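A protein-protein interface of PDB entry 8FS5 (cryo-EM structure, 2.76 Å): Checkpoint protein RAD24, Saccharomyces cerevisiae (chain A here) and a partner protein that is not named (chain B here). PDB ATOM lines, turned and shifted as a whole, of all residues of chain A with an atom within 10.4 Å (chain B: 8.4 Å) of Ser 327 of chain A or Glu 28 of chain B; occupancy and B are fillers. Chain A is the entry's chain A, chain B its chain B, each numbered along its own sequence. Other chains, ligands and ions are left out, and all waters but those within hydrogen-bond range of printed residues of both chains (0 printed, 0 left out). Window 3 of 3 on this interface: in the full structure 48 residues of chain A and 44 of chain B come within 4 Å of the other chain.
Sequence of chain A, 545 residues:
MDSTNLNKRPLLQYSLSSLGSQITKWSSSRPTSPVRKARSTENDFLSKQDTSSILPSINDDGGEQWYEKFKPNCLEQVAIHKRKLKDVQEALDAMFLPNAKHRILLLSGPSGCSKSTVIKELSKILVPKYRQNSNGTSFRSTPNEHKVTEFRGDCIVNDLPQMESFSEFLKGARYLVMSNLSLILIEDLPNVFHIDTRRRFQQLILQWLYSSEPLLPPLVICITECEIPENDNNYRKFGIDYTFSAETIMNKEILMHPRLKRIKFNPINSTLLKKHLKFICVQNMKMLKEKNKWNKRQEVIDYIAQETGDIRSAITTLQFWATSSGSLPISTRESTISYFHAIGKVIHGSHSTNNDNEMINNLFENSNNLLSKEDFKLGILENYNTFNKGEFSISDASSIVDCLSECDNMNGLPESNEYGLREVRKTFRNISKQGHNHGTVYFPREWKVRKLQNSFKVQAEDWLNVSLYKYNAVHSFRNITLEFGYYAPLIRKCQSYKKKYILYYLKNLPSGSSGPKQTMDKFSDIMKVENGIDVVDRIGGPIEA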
ATOM      1  N   LYS A 291       4.096 -14.689 -36.383  1.00  0.00           N
ATOM      2  CA  LYS A 291       3.859 -15.718 -35.376  1.00  0.00           C
ATOM      3  C   LYS A 291       3.277 -15.115 -34.105  1.00  0.00           C
ATOM      4  O   LYS A 291       3.450 -15.673 -33.015  1.00  0.00           O
ATOM      5  CB  LYS A 291       5.152 -16.473 -35.060  1.00  0.00           C
ATOM      6  CG  LYS A 291       5.758 -17.196 -36.248  1.00  0.00           C
ATOM      7  CD  LYS A 291       6.868 -18.136 -35.806  1.00  0.00           C
ATOM      8  CE  LYS A 291       7.421 -18.932 -36.977  1.00  0.00           C
ATOM      9  NZ  LYS A 291       8.464 -19.902 -36.542  1.00  0.00           N
ATOM     10  N   ASN A 292       2.599 -13.971 -34.252  1.00  0.00           N
ATOM     11  CA  ASN A 292       1.962 -13.214 -33.165  1.00  0.00           C
ATOM     12  C   ASN A 292       2.864 -13.083 -31.938  1.00  0.00           C
ATOM     13  O   ASN A 292       2.405 -13.116 -30.794  1.00  0.00           O
ATOM     14  CB  ASN A 292       0.591 -13.802 -32.789  1.00  0.00           C
ATOM     15  CG  ASN A 292       0.666 -15.228 -32.270  1.00  0.00           C
ATOM     16  OD1 ASN A 292       0.970 -15.463 -31.100  1.00  0.00           O
ATOM     17  ND2 ASN A 292       0.380 -16.188 -33.141  1.00  0.00           N
ATOM     18  N   LYS A 293       4.167 -12.905 -32.177  1.00  0.00           N
ATOM     19  CA  LYS A 293       5.128 -12.635 -31.111  1.00  0.00           C
ATOM     20  C   LYS A 293       5.922 -11.366 -31.462  1.00  0.00           C
ATOM     21  O   LYS A 293       7.045 -11.392 -31.964  1.00  0.00           O
ATOM     22  CB  LYS A 293       6.021 -13.870 -30.855  1.00  0.00           C
ATOM     23  CG  LYS A 293       6.895 -14.347 -32.022  1.00  0.00           C
ATOM     24  CD  LYS A 293       7.459 -15.748 -31.795  1.00  0.00           C
ATOM     25  CE  LYS A 293       6.559 -16.598 -30.911  1.00  0.00           C
ATOM     26  NZ  LYS A 293       7.230 -17.857 -30.491  1.00  0.00           N
ATOM     27  N   LYS A 296       5.068  -9.289 -26.950  1.00  0.00           N
ATOM     28  CA  LYS A 296       5.750  -9.932 -25.835  1.00  0.00           C
ATOM     29  C   LYS A 296       7.248 -10.058 -26.060  1.00  0.00           C
ATOM     30  O   LYS A 296       7.906 -10.808 -25.332  1.00  0.00           O
ATOM     31  CB  LYS A 296       5.153 -11.317 -25.567  1.00  0.00           C
ATOM     32  CG  LYS A 296       4.497 -11.985 -26.765  1.00  0.00           C
ATOM     33  CD  LYS A 296       3.587 -13.116 -26.304  1.00  0.00           C
ATOM     34  CE  LYS A 296       2.689 -13.621 -27.421  1.00  0.00           C
ATOM     35  NZ  LYS A 296       3.464 -14.046 -28.616  1.00  0.00           N
ATOM     36  N   VAL A 300      10.694 -10.972 -23.100  1.00  0.00           N
ATOM     37  CA  VAL A 300      11.669 -12.040 -23.309  1.00  0.00           C
ATOM     38  C   VAL A 300      13.076 -11.462 -23.447  1.00  0.00           C
ATOM     39  O   VAL A 300      14.044 -12.038 -22.936  1.00  0.00           O
ATOM     40  CB  VAL A 300      11.285 -12.932 -24.507  1.00  0.00           C
ATOM     41  CG1 VAL A 300      10.044 -13.752 -24.182  1.00  0.00           C
ATOM     42  CG2 VAL A 300      11.084 -12.138 -25.773  1.00  0.00           C
ATOM     43  N   PHE A 320      15.716 -19.540 -30.748  1.00  0.00           N
ATOM     44  CA  PHE A 320      14.932 -20.723 -30.412  1.00  0.00           C
ATOM     45  C   PHE A 320      13.519 -20.357 -29.977  1.00  0.00           C
ATOM     46  O   PHE A 320      12.564 -21.061 -30.323  1.00  0.00           O
ATOM     47  CB  PHE A 320      15.636 -21.525 -29.317  1.00  0.00           C
ATOM     48  CG  PHE A 320      15.191 -22.955 -29.234  1.00  0.00           C
ATOM     49  CD1 PHE A 320      15.695 -23.902 -30.111  1.00  0.00           C
ATOM     50  CD2 PHE A 320      14.268 -23.355 -28.283  1.00  0.00           C
ATOM     51  CE1 PHE A 320      15.288 -25.220 -30.039  1.00  0.00           C
ATOM     52  CE2 PHE A 320      13.856 -24.672 -28.206  1.00  0.00           C
ATOM     53  CZ  PHE A 320      14.367 -25.605 -29.086  1.00  0.00           C
ATOM     54  N   TRP A 321      13.365 -19.268 -29.222  1.00  0.00           N
ATOM     55  CA  TRP A 321      12.042 -18.810 -28.817  1.00  0.00           C
ATOM     56  C   TRP A 321      11.239 -18.255 -29.988  1.00  0.00           C
ATOM     57  O   TRP A 321      10.029 -18.488 -30.071  1.00  0.00           O
ATOM     58  CB  TRP A 321      12.166 -17.750 -27.716  1.00  0.00           C
ATOM     59  CG  TRP A 321      10.971 -16.847 -27.599  1.00  0.00           C
ATOM     60  CD1 TRP A 321       9.840 -17.077 -26.871  1.00  0.00           C
ATOM     61  CD2 TRP A 321      10.794 -15.568 -28.220  1.00  0.00           C
ATOM     62  NE1 TRP A 321       8.968 -16.024 -27.005  1.00  0.00           N
ATOM     63  CE2 TRP A 321       9.530 -15.085 -27.828  1.00  0.00           C
ATOM     64  CE3 TRP A 321      11.579 -14.786 -29.074  1.00  0.00           C
ATOM     65  CZ2 TRP A 321       9.034 -13.856 -28.259  1.00  0.00           C
ATOM     66  CZ3 TRP A 321      11.085 -13.567 -29.500  1.00  0.00           C
ATOM     67  CH2 TRP A 321       9.825 -13.113 -29.092  1.00  0.00           C
ATOM     68  N   ALA A 322      11.890 -17.523 -30.896  1.00  0.00           N
ATOM     69  CA  ALA A 322      11.177 -16.931 -32.024  1.00  0.00           C
ATOM     70  C   ALA A 322      10.710 -17.999 -33.005  1.00  0.00           C
ATOM     71  O   ALA A 322       9.552 -17.998 -33.435  1.00  0.00           O
ATOM     72  CB  ALA A 322      12.069 -15.906 -32.725  1.00  0.00           C
ATOM     73  N   THR A 323      11.596 -18.933 -33.358  1.00  0.00           N
ATOM     74  CA  THR A 323      11.238 -19.980 -34.309  1.00  0.00           C
ATOM     75  C   THR A 323      10.270 -21.004 -33.731  1.00  0.00           C
ATOM     76  O   THR A 323       9.792 -21.865 -34.477  1.00  0.00           O
ATOM     77  CB  THR A 323      12.495 -20.689 -34.818  1.00  0.00           C
ATOM     78  OG1 THR A 323      13.184 -21.297 -33.717  1.00  0.00           O
ATOM     79  CG2 THR A 323      13.420 -19.704 -35.517  1.00  0.00           C
ATOM     80  N   SER A 324       9.972 -20.936 -32.438  1.00  0.00           N
ATOM     81  CA  SER A 324       9.030 -21.832 -31.794  1.00  0.00           C
ATOM     82  C   SER A 324       7.602 -21.360 -32.063  1.00  0.00           C
ATOM     83  O   SER A 324       7.368 -20.236 -32.520  1.00  0.00           O
ATOM     84  CB  SER A 324       9.327 -21.910 -30.295  1.00  0.00           C
ATOM     85  OG  SER A 324       8.325 -22.646 -29.615  1.00  0.00           O
ATOM     86  N   SER A 325       6.632 -22.228 -31.782  1.00  0.00           N
ATOM     87  CA  SER A 325       5.226 -21.887 -31.955  1.00  0.00           C
ATOM     88  C   SER A 325       4.404 -22.399 -30.781  1.00  0.00           C
ATOM     89  O   SER A 325       3.230 -22.748 -30.940  1.00  0.00           O
ATOM     90  CB  SER A 325       4.693 -22.457 -33.271  1.00  0.00           C
ATOM     91  OG  SER A 325       3.326 -22.130 -33.452  1.00  0.00           O
ATOM     92  N   GLY A 326       5.009 -22.449 -29.605  1.00  0.00           N
ATOM     93  CA  GLY A 326       4.335 -22.954 -28.434  1.00  0.00           C
ATOM     94  C   GLY A 326       4.696 -22.173 -27.193  1.00  0.00           C
ATOM     95  O   GLY A 326       5.210 -21.056 -27.265  1.00  0.00           O
ATOM     96  N   SER A 327       4.453 -22.771 -26.025  1.00  0.00           N
ATOM     97  CA  SER A 327       4.714 -22.118 -24.723  1.00  0.00           C
ATOM     98  C   SER A 327       5.912 -22.769 -24.032  1.00  0.00           C
ATOM     99  O   SER A 327       5.951 -22.732 -22.788  1.00  0.00           O
ATOM    100  CB  SER A 327       3.492 -22.183 -23.861  1.00  0.00           C
ATOM    101  OG  SER A 327       2.371 -21.638 -24.539  1.00  0.00           O
ATOM    102  N   LEU A 328       6.849 -23.342 -24.790  1.00  0.00           N
ATOM    103  CA  LEU A 328       8.087 -23.905 -24.198  1.00  0.00           C
ATOM    104  C   LEU A 328       8.741 -22.779 -23.393  1.00  0.00           C
ATOM    105  O   LEU A 328       8.711 -21.630 -23.865  1.00  0.00           O
ATOM    106  CB  LEU A 328       8.996 -24.425 -25.314  1.00  0.00           C
ATOM    107  CG  LEU A 328      10.099 -25.390 -24.884  1.00  0.00           C
ATOM    108  CD1 LEU A 328       9.513 -26.636 -24.247  1.00  0.00           C
ATOM    109  CD2 LEU A 328      10.968 -25.770 -26.069  1.00  0.00           C
ATOM    110  N   PRO A 329       9.302 -23.037 -22.193  1.00  0.00           N
ATOM    111  CA  PRO A 329       9.849 -21.971 -21.349  1.00  0.00           C
ATOM    112  C   PRO A 329      11.242 -21.486 -21.772  1.00  0.00           C
ATOM    113  O   PRO A 329      12.008 -22.294 -22.260  1.00  0.00           O
ATOM    114  CB  PRO A 329       9.945 -22.658 -19.981  1.00  0.00           C
ATOM    115  CG  PRO A 329      10.261 -24.092 -20.329  1.00  0.00           C
ATOM    116  CD  PRO A 329       9.464 -24.362 -21.589  1.00  0.00           C
ATOM    117  N   ILE A 330      11.546 -20.203 -21.562  1.00  0.00           N
ATOM    118  CA  ILE A 330      12.873 -19.623 -21.912  1.00  0.00           C
ATOM    119  C   ILE A 330      13.899 -20.173 -20.927  1.00  0.00           C
ATOM    120  O   ILE A 330      13.718 -19.957 -19.718  1.00  0.00           O
ATOM    121  CB  ILE A 330      12.837 -18.084 -21.934  1.00  0.00           C
ATOM    122  CG1 ILE A 330      11.824 -17.558 -22.950  1.00  0.00           C
ATOM    123  CG2 ILE A 330      14.224 -17.516 -22.185  1.00  0.00           C
ATOM    124  CD1 ILE A 330      10.647 -16.857 -22.327  1.00  0.00           C
ATOM    125  N   SER A 331      14.922 -20.859 -21.417  1.00  0.00           N
ATOM    126  CA  SER A 331      16.004 -21.467 -20.651  1.00  0.00           C
ATOM    127  C   SER A 331      17.322 -21.184 -21.351  1.00  0.00           C
ATOM    128  O   SER A 331      17.497 -21.545 -22.520  1.00  0.00           O
ATOM    129  CB  SER A 331      15.791 -22.976 -20.494  1.00  0.00           C
ATOM    130  OG  SER A 331      16.879 -23.576 -19.813  1.00  0.00           O
ATOM    131  N   GLY B  25       4.925 -37.271 -22.030  1.00  0.00           N
ATOM    132  CA  GLY B  25       5.611 -36.365 -21.134  1.00  0.00           C
ATOM    133  C   GLY B  25       6.378 -35.282 -21.871  1.00  0.00           C
ATOM    134  O   GLY B  25       6.837 -35.451 -23.003  1.00  0.00           O
ATOM    135  N   ASN B  26       6.523 -34.145 -21.194  1.00  0.00           N
ATOM    136  CA  ASN B  26       7.186 -32.957 -21.732  1.00  0.00           C
ATOM    137  C   ASN B  26       6.564 -32.549 -23.066  1.00  0.00           C
ATOM    138  O   ASN B  26       7.208 -32.544 -24.115  1.00  0.00           O
ATOM    139  CB  ASN B  26       8.692 -33.181 -21.870  1.00  0.00           C
ATOM    140  CG  ASN B  26       9.337 -33.625 -20.572  1.00  0.00           C
ATOM    141  OD1 ASN B  26       9.490 -32.837 -19.640  1.00  0.00           O
ATOM    142  ND2 ASN B  26       9.720 -34.894 -20.507  1.00  0.00           N
ATOM    143  N   LYS B  27       5.275 -32.201 -22.999  1.00  0.00           N
ATOM    144  CA  LYS B  27       4.487 -31.994 -24.211  1.00  0.00           C
ATOM    145  C   LYS B  27       5.034 -30.844 -25.048  1.00  0.00           C
ATOM    146  O   LYS B  27       5.121 -30.944 -26.276  1.00  0.00           O
ATOM    147  CB  LYS B  27       3.024 -31.744 -23.842  1.00  0.00           C
ATOM    148  CG  LYS B  27       2.028 -32.304 -24.844  1.00  0.00           C
ATOM    149  CD  LYS B  27       0.766 -31.461 -24.901  1.00  0.00           C
ATOM    150  CE  LYS B  27      -0.146 -31.911 -26.031  1.00  0.00           C
ATOM    151  NZ  LYS B  27       0.619 -32.520 -27.154  1.00  0.00           N
ATOM    152  N   GLU B  28       5.407 -29.737 -24.399  1.00  0.00           N
ATOM    153  CA  GLU B  28       5.934 -28.592 -25.136  1.00  0.00           C
ATOM    154  C   GLU B  28       7.259 -28.915 -25.818  1.00  0.00           C
ATOM    155  O   GLU B  28       7.461 -28.545 -26.980  1.00  0.00           O
ATOM    156  CB  GLU B  28       6.095 -27.394 -24.201  1.00  0.00           C
ATOM    157  CG  GLU B  28       5.028 -27.303 -23.122  1.00  0.00           C
ATOM    158  CD  GLU B  28       5.546 -26.676 -21.841  1.00  0.00           C
ATOM    159  OE1 GLU B  28       6.550 -27.179 -21.294  1.00  0.00           O
ATOM    160  OE2 GLU B  28       4.948 -25.680 -21.383  1.00  0.00           O
ATOM    161  N   THR B  29       8.164 -29.604 -25.121  1.00  0.00           N
ATOM    162  CA  THR B  29       9.457 -29.942 -25.709  1.00  0.00           C
ATOM    163  C   THR B  29       9.315 -30.939 -26.854  1.00  0.00           C
ATOM    164  O   THR B  29      10.000 -30.815 -27.874  1.00  0.00           O
ATOM    165  CB  THR B  29      10.397 -30.492 -24.637  1.00  0.00           C
ATOM    166  OG1 THR B  29      10.251 -29.729 -23.434  1.00  0.00           O
ATOM    167  CG2 THR B  29      11.839 -30.400 -25.107  1.00  0.00           C
ATOM    168  N   ILE B  30       8.432 -31.930 -26.707  1.00  0.00           N
ATOM    169  CA  ILE B  30       8.204 -32.880 -27.792  1.00  0.00           C
ATOM    170  C   ILE B  30       7.545 -32.192 -28.982  1.00  0.00           C
ATOM    171  O   ILE B  30       7.868 -32.491 -30.139  1.00  0.00           O
ATOM    172  CB  ILE B  30       7.374 -34.076 -27.290  1.00  0.00           C
ATOM    173  CG1 ILE B  30       8.107 -34.793 -26.153  1.00  0.00           C
ATOM    174  CG2 ILE B  30       7.085 -35.048 -28.420  1.00  0.00           C
ATOM    175  CD1 ILE B  30       9.418 -35.423 -26.571  1.00  0.00           C
ATOM    176  N   ASP B  31       6.627 -31.254 -28.729  1.00  0.00           N
ATOM    177  CA  ASP B  31       6.028 -30.491 -29.819  1.00  0.00           C
ATOM    178  C   ASP B  31       7.081 -29.669 -30.552  1.00  0.00           C
ATOM    179  O   ASP B  31       7.097 -29.618 -31.788  1.00  0.00           O
ATOM    180  CB  ASP B  31       4.917 -29.592 -29.279  1.00  0.00           C
ATOM    181  CG  ASP B  31       3.646 -30.358 -28.968  1.00  0.00           C
ATOM    182  OD1 ASP B  31       3.455 -31.451 -29.540  1.00  0.00           O
ATOM    183  OD2 ASP B  31       2.839 -29.867 -28.150  1.00  0.00           O
ATOM    184  N   ARG B  32       7.981 -29.026 -29.802  1.00  0.00           N
ATOM    185  CA  ARG B  32       9.068 -28.274 -30.423  1.00  0.00           C
ATOM    186  C   ARG B  32       9.989 -29.181 -31.228  1.00  0.00           C
ATOM    187  O   ARG B  32      10.452 -28.796 -32.309  1.00  0.00           O
ATOM    188  CB  ARG B  32       9.862 -27.521 -29.357  1.00  0.00           C
ATOM    189  CG  ARG B  32      10.975 -26.651 -29.916  1.00  0.00           C
ATOM    190  CD  ARG B  32      10.432 -25.346 -30.465  1.00  0.00           C
ATOM    191  NE  ARG B  32      11.499 -24.453 -30.903  1.00  0.00           N
ATOM    192  CZ  ARG B  32      11.981 -24.412 -32.138  1.00  0.00           C
ATOM    193  NH1 ARG B  32      11.513 -25.203 -33.089  1.00  0.00           N
ATOM    194  NH2 ARG B  32      12.958 -23.557 -32.424  1.00  0.00           N
ATOM    195  N   LEU B  33      10.272 -30.382 -30.718  1.00  0.00           N
ATOM    196  CA  LEU B  33      11.065 -31.341 -31.480  1.00  0.00           C
ATOM    197  C   LEU B  33      10.351 -31.743 -32.765  1.00  0.00           C
ATOM    198  O   LEU B  33      10.995 -31.968 -33.794  1.00  0.00           O
ATOM    199  CB  LEU B  33      11.370 -32.569 -30.624  1.00  0.00           C
ATOM    200  CG  LEU B  33      12.491 -32.426 -29.591  1.00  0.00           C
ATOM    201  CD1 LEU B  33      12.971 -33.793 -29.129  1.00  0.00           C
ATOM    202  CD2 LEU B  33      13.649 -31.607 -30.145  1.00  0.00           C
ATOM    203  N   GLN B  34       9.020 -31.837 -32.723  1.00  0.00           N
ATOM    204  CA  GLN B  34       8.261 -32.128 -33.937  1.00  0.00           C
ATOM    205  C   GLN B  34       8.358 -30.982 -34.944  1.00  0.00           C
ATOM    206  O   GLN B  34       8.468 -31.218 -36.155  1.00  0.00           O
ATOM    207  CB  GLN B  34       6.802 -32.418 -33.588  1.00  0.00           C
ATOM    208  CG  GLN B  34       6.462 -33.900 -33.559  1.00  0.00           C
ATOM    209  CD  GLN B  34       5.410 -34.239 -32.524  1.00  0.00           C
ATOM    210  OE1 GLN B  34       5.086 -33.423 -31.660  1.00  0.00           O
ATOM    211  NE2 GLN B  34       4.868 -35.448 -32.605  1.00  0.00           N
ATOM    212  N   GLN B  35       8.301 -29.735 -34.463  1.00  0.00           N
ATOM    213  CA  GLN B  35       8.498 -28.596 -35.361  1.00  0.00           C
ATOM    214  C   GLN B  35       9.892 -28.622 -35.979  1.00  0.00           C
ATOM    215  O   GLN B  35      10.061 -28.331 -37.167  1.00  0.00           O
ATOM    216  CB  GLN B  35       8.266 -27.265 -34.639  1.00  0.00           C
ATOM    217  CG  GLN B  35       7.117 -27.236 -33.658  1.00  0.00           C
ATOM    218  CD  GLN B  35       6.960 -25.886 -32.986  1.00  0.00           C
ATOM    219  OE1 GLN B  35       7.481 -24.878 -33.462  1.00  0.00           O
ATOM    220  NE2 GLN B  35       6.239 -25.860 -31.871  1.00  0.00           N
ATOM    221  N   LEU B 161      17.707 -27.707 -23.680  1.00  0.00           N
ATOM    222  CA  LEU B 161      16.357 -28.240 -23.519  1.00  0.00           C
ATOM    223  C   LEU B 161      16.354 -29.141 -22.292  1.00  0.00           C
ATOM    224  O   LEU B 161      16.967 -30.213 -22.301  1.00  0.00           O
ATOM    225  CB  LEU B 161      15.913 -29.007 -24.763  1.00  0.00           C
ATOM    226  CG  LEU B 161      15.686 -28.185 -26.034  1.00  0.00           C
ATOM    227  CD1 LEU B 161      15.742 -29.074 -27.264  1.00  0.00           C
ATOM    228  CD2 LEU B 161      14.357 -27.453 -25.958  1.00  0.00           C
ATOM    229  N   ARG B 162      15.665 -28.711 -21.239  1.00  0.00           N
ATOM    230  CA  ARG B 162      15.628 -29.438 -19.977  1.00  0.00           C
ATOM    231  C   ARG B 162      14.356 -30.273 -19.912  1.00  0.00           C
ATOM    232  O   ARG B 162      13.248 -29.735 -20.013  1.00  0.00           O
ATOM    233  CB  ARG B 162      15.704 -28.474 -18.794  1.00  0.00           C
ATOM    234  CG  ARG B 162      16.946 -27.599 -18.801  1.00  0.00           C
ATOM    235  CD  ARG B 162      17.077 -26.792 -17.521  1.00  0.00           C
ATOM    236  NE  ARG B 162      17.825 -25.560 -17.735  1.00  0.00           N
ATOM    237  CZ  ARG B 162      19.147 -25.466 -17.677  1.00  0.00           C
ATOM    238  NH1 ARG B 162      19.904 -26.519 -17.412  1.00  0.00           N
ATOM    239  NH2 ARG B 162      19.724 -24.287 -17.892  1.00  0.00           N
ATOM    240  N   TYR B 163      14.519 -31.583 -19.746  1.00  0.00           N
ATOM    241  CA  TYR B 163      13.396 -32.505 -19.646  1.00  0.00           C
ATOM    242  C   TYR B 163      13.013 -32.665 -18.181  1.00  0.00           C
ATOM    243  O   TYR B 163      13.847 -33.048 -17.354  1.00  0.00           O
ATOM    244  CB  TYR B 163      13.750 -33.858 -20.259  1.00  0.00           C
ATOM    245  CG  TYR B 163      13.491 -33.967 -21.744  1.00  0.00           C
ATOM    246  CD1 TYR B 163      14.015 -33.036 -22.631  1.00  0.00           C
ATOM    247  CD2 TYR B 163      12.727 -35.005 -22.261  1.00  0.00           C
ATOM    248  CE1 TYR B 163      13.784 -33.137 -23.990  1.00  0.00           C
ATOM    249  CE2 TYR B 163      12.489 -35.112 -23.616  1.00  0.00           C
ATOM    250  CZ  TYR B 163      13.019 -34.175 -24.477  1.00  0.00           C
ATOM    251  OH  TYR B 163      12.784 -34.278 -25.828  1.00  0.00           O
ATOM    252  N   SER B 164      11.755 -32.371 -17.861  1.00  0.00           N
ATOM    253  CA  SER B 164      11.275 -32.484 -16.495  1.00  0.00           C
ATOM    254  C   SER B 164      10.866 -33.921 -16.184  1.00  0.00           C
ATOM    255  O   SER B 164      10.847 -34.794 -17.055  1.00  0.00           O
ATOM    256  CB  SER B 164      10.098 -31.537 -16.260  1.00  0.00           C
ATOM    257  OG  SER B 164      10.430 -30.210 -16.629  1.00  0.00           O
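The backbone carbonyl oxygen (O) of Ser 327 of chain A lies close to the side-chain carboxylate (OE2) of Glu 28 of chain B, 3.4 Å away.
The side-chain hydroxyl (OG1) of Thr 323 of chain A sits at hydrogen-bond distance from the guanidinium group (NH2) of Arg 32 of chain B (2.6 Å).
OG of Ser 331 of chain A lies within hydrogen-bond range of NE of Arg 162 of chain B (3.0 Å).
O of Phe 320 of chain A is in hydrogen-bond range of NH2 of Arg 32 of chain B.
The backbone NH (N) of Ser 325 of chain A sits at hydrogen-bond distance from the side-chain amide oxygen (OE1) of Gln 35 of chain B, 3.3 Å away.
OG1 of Thr 323 of chain A is in hydrogen-bond range of O of Phe 320 of chain A, 3.5 Å away.
The backbone carbonyl oxygen of Ser 324 of chain A sits at hydrogen-bond distance from the side-chain amino group of Lys 293 of chain A, at 3.1 Å.
The backbone NH (N) of Gly 326 of chain A lies within hydrogen-bond range of the side-chain hydroxyl (OG) of Ser 324 of chain A.
NZ of Lys 291 of chain A is in hydrogen-bond range of O of Thr 323 of chain A (3.1 Å).
Among the printed residues, merely in contact across the chains: Leu 328 of chain A with Thr 29 of chain B (3.3 Å), Ser 324 of chain A with Arg 32 of chain B (3.4 Å), Leu 328 of chain A with Glu 28 of chain B (3.5 Å), Phe 320 of chain A with Leu 161 of chain B (3.6 Å), Leu 328 of chain A with Leu 161 of chain B (3.8 Å), Ser 324 of chain A with Gln 35 of chain B (3.8 Å), Leu 328 of chain A with Arg 32 of chain B (3.9 Å) and Thr 323 of chain A with Gln 35 of chain B (3.9 Å).
Of chain B, only Glu 28 (3.4 Å) comes within 4 Å of Ser 327 of chain A.
Of chain A, only Ser 327 (3.4 Å) and Leu 328 (3.5 Å) come within 4 Å of Glu 28 of chain B.
Gly 326 of chain A touches none of the printed residues of chain B.
No residue of chain A comes within 4 Å of Lys 27 of chain B.
No residue of chain A comes within 4 Å of Asp 31 of chain B.
Printed residues of chain A within 4 Å of Arg 32 of chain B: Phe 320 (3.3 Å), Thr 323 (2.6 Å), Ser 324 (3.4 Å) and Leu 328 (3.9 Å).
Printed residues of chain A within 4 Å of Leu 161 of chain B: Phe 320 (3.6 Å) and Leu 328 (3.8 Å).
Printed residues of chain A within 4 Å of Arg 162 of chain B: Ser 331.
The nearest residue of chain B that does not touch Ser 327 of chain A is Gln 35 of chain B (6.8 Å).
Hydrophobic or aromatic side chains of chain B within 4 Å of the printed part of chain A: Leu 161.
Of the 17 printed residues of chain A, 7 touch a printed residue of chain B.
Printed residues of chain A that touch a printed residue of chain B: Phe 320, Thr 323, Ser 324, Ser 325, Ser 327, Leu 328 and Ser 331.
Hydrophobic or aromatic side chains of chain A within 4 Å of the printed part of chain B: Phe 320 and Leu 328.
Among the printed residues, 13 pairs touch across the chains.
Among the printed residues, no Asp or Glu carboxylate lies within 4 Å of a Lys or Arg side-chain nitrogen of the other chain.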
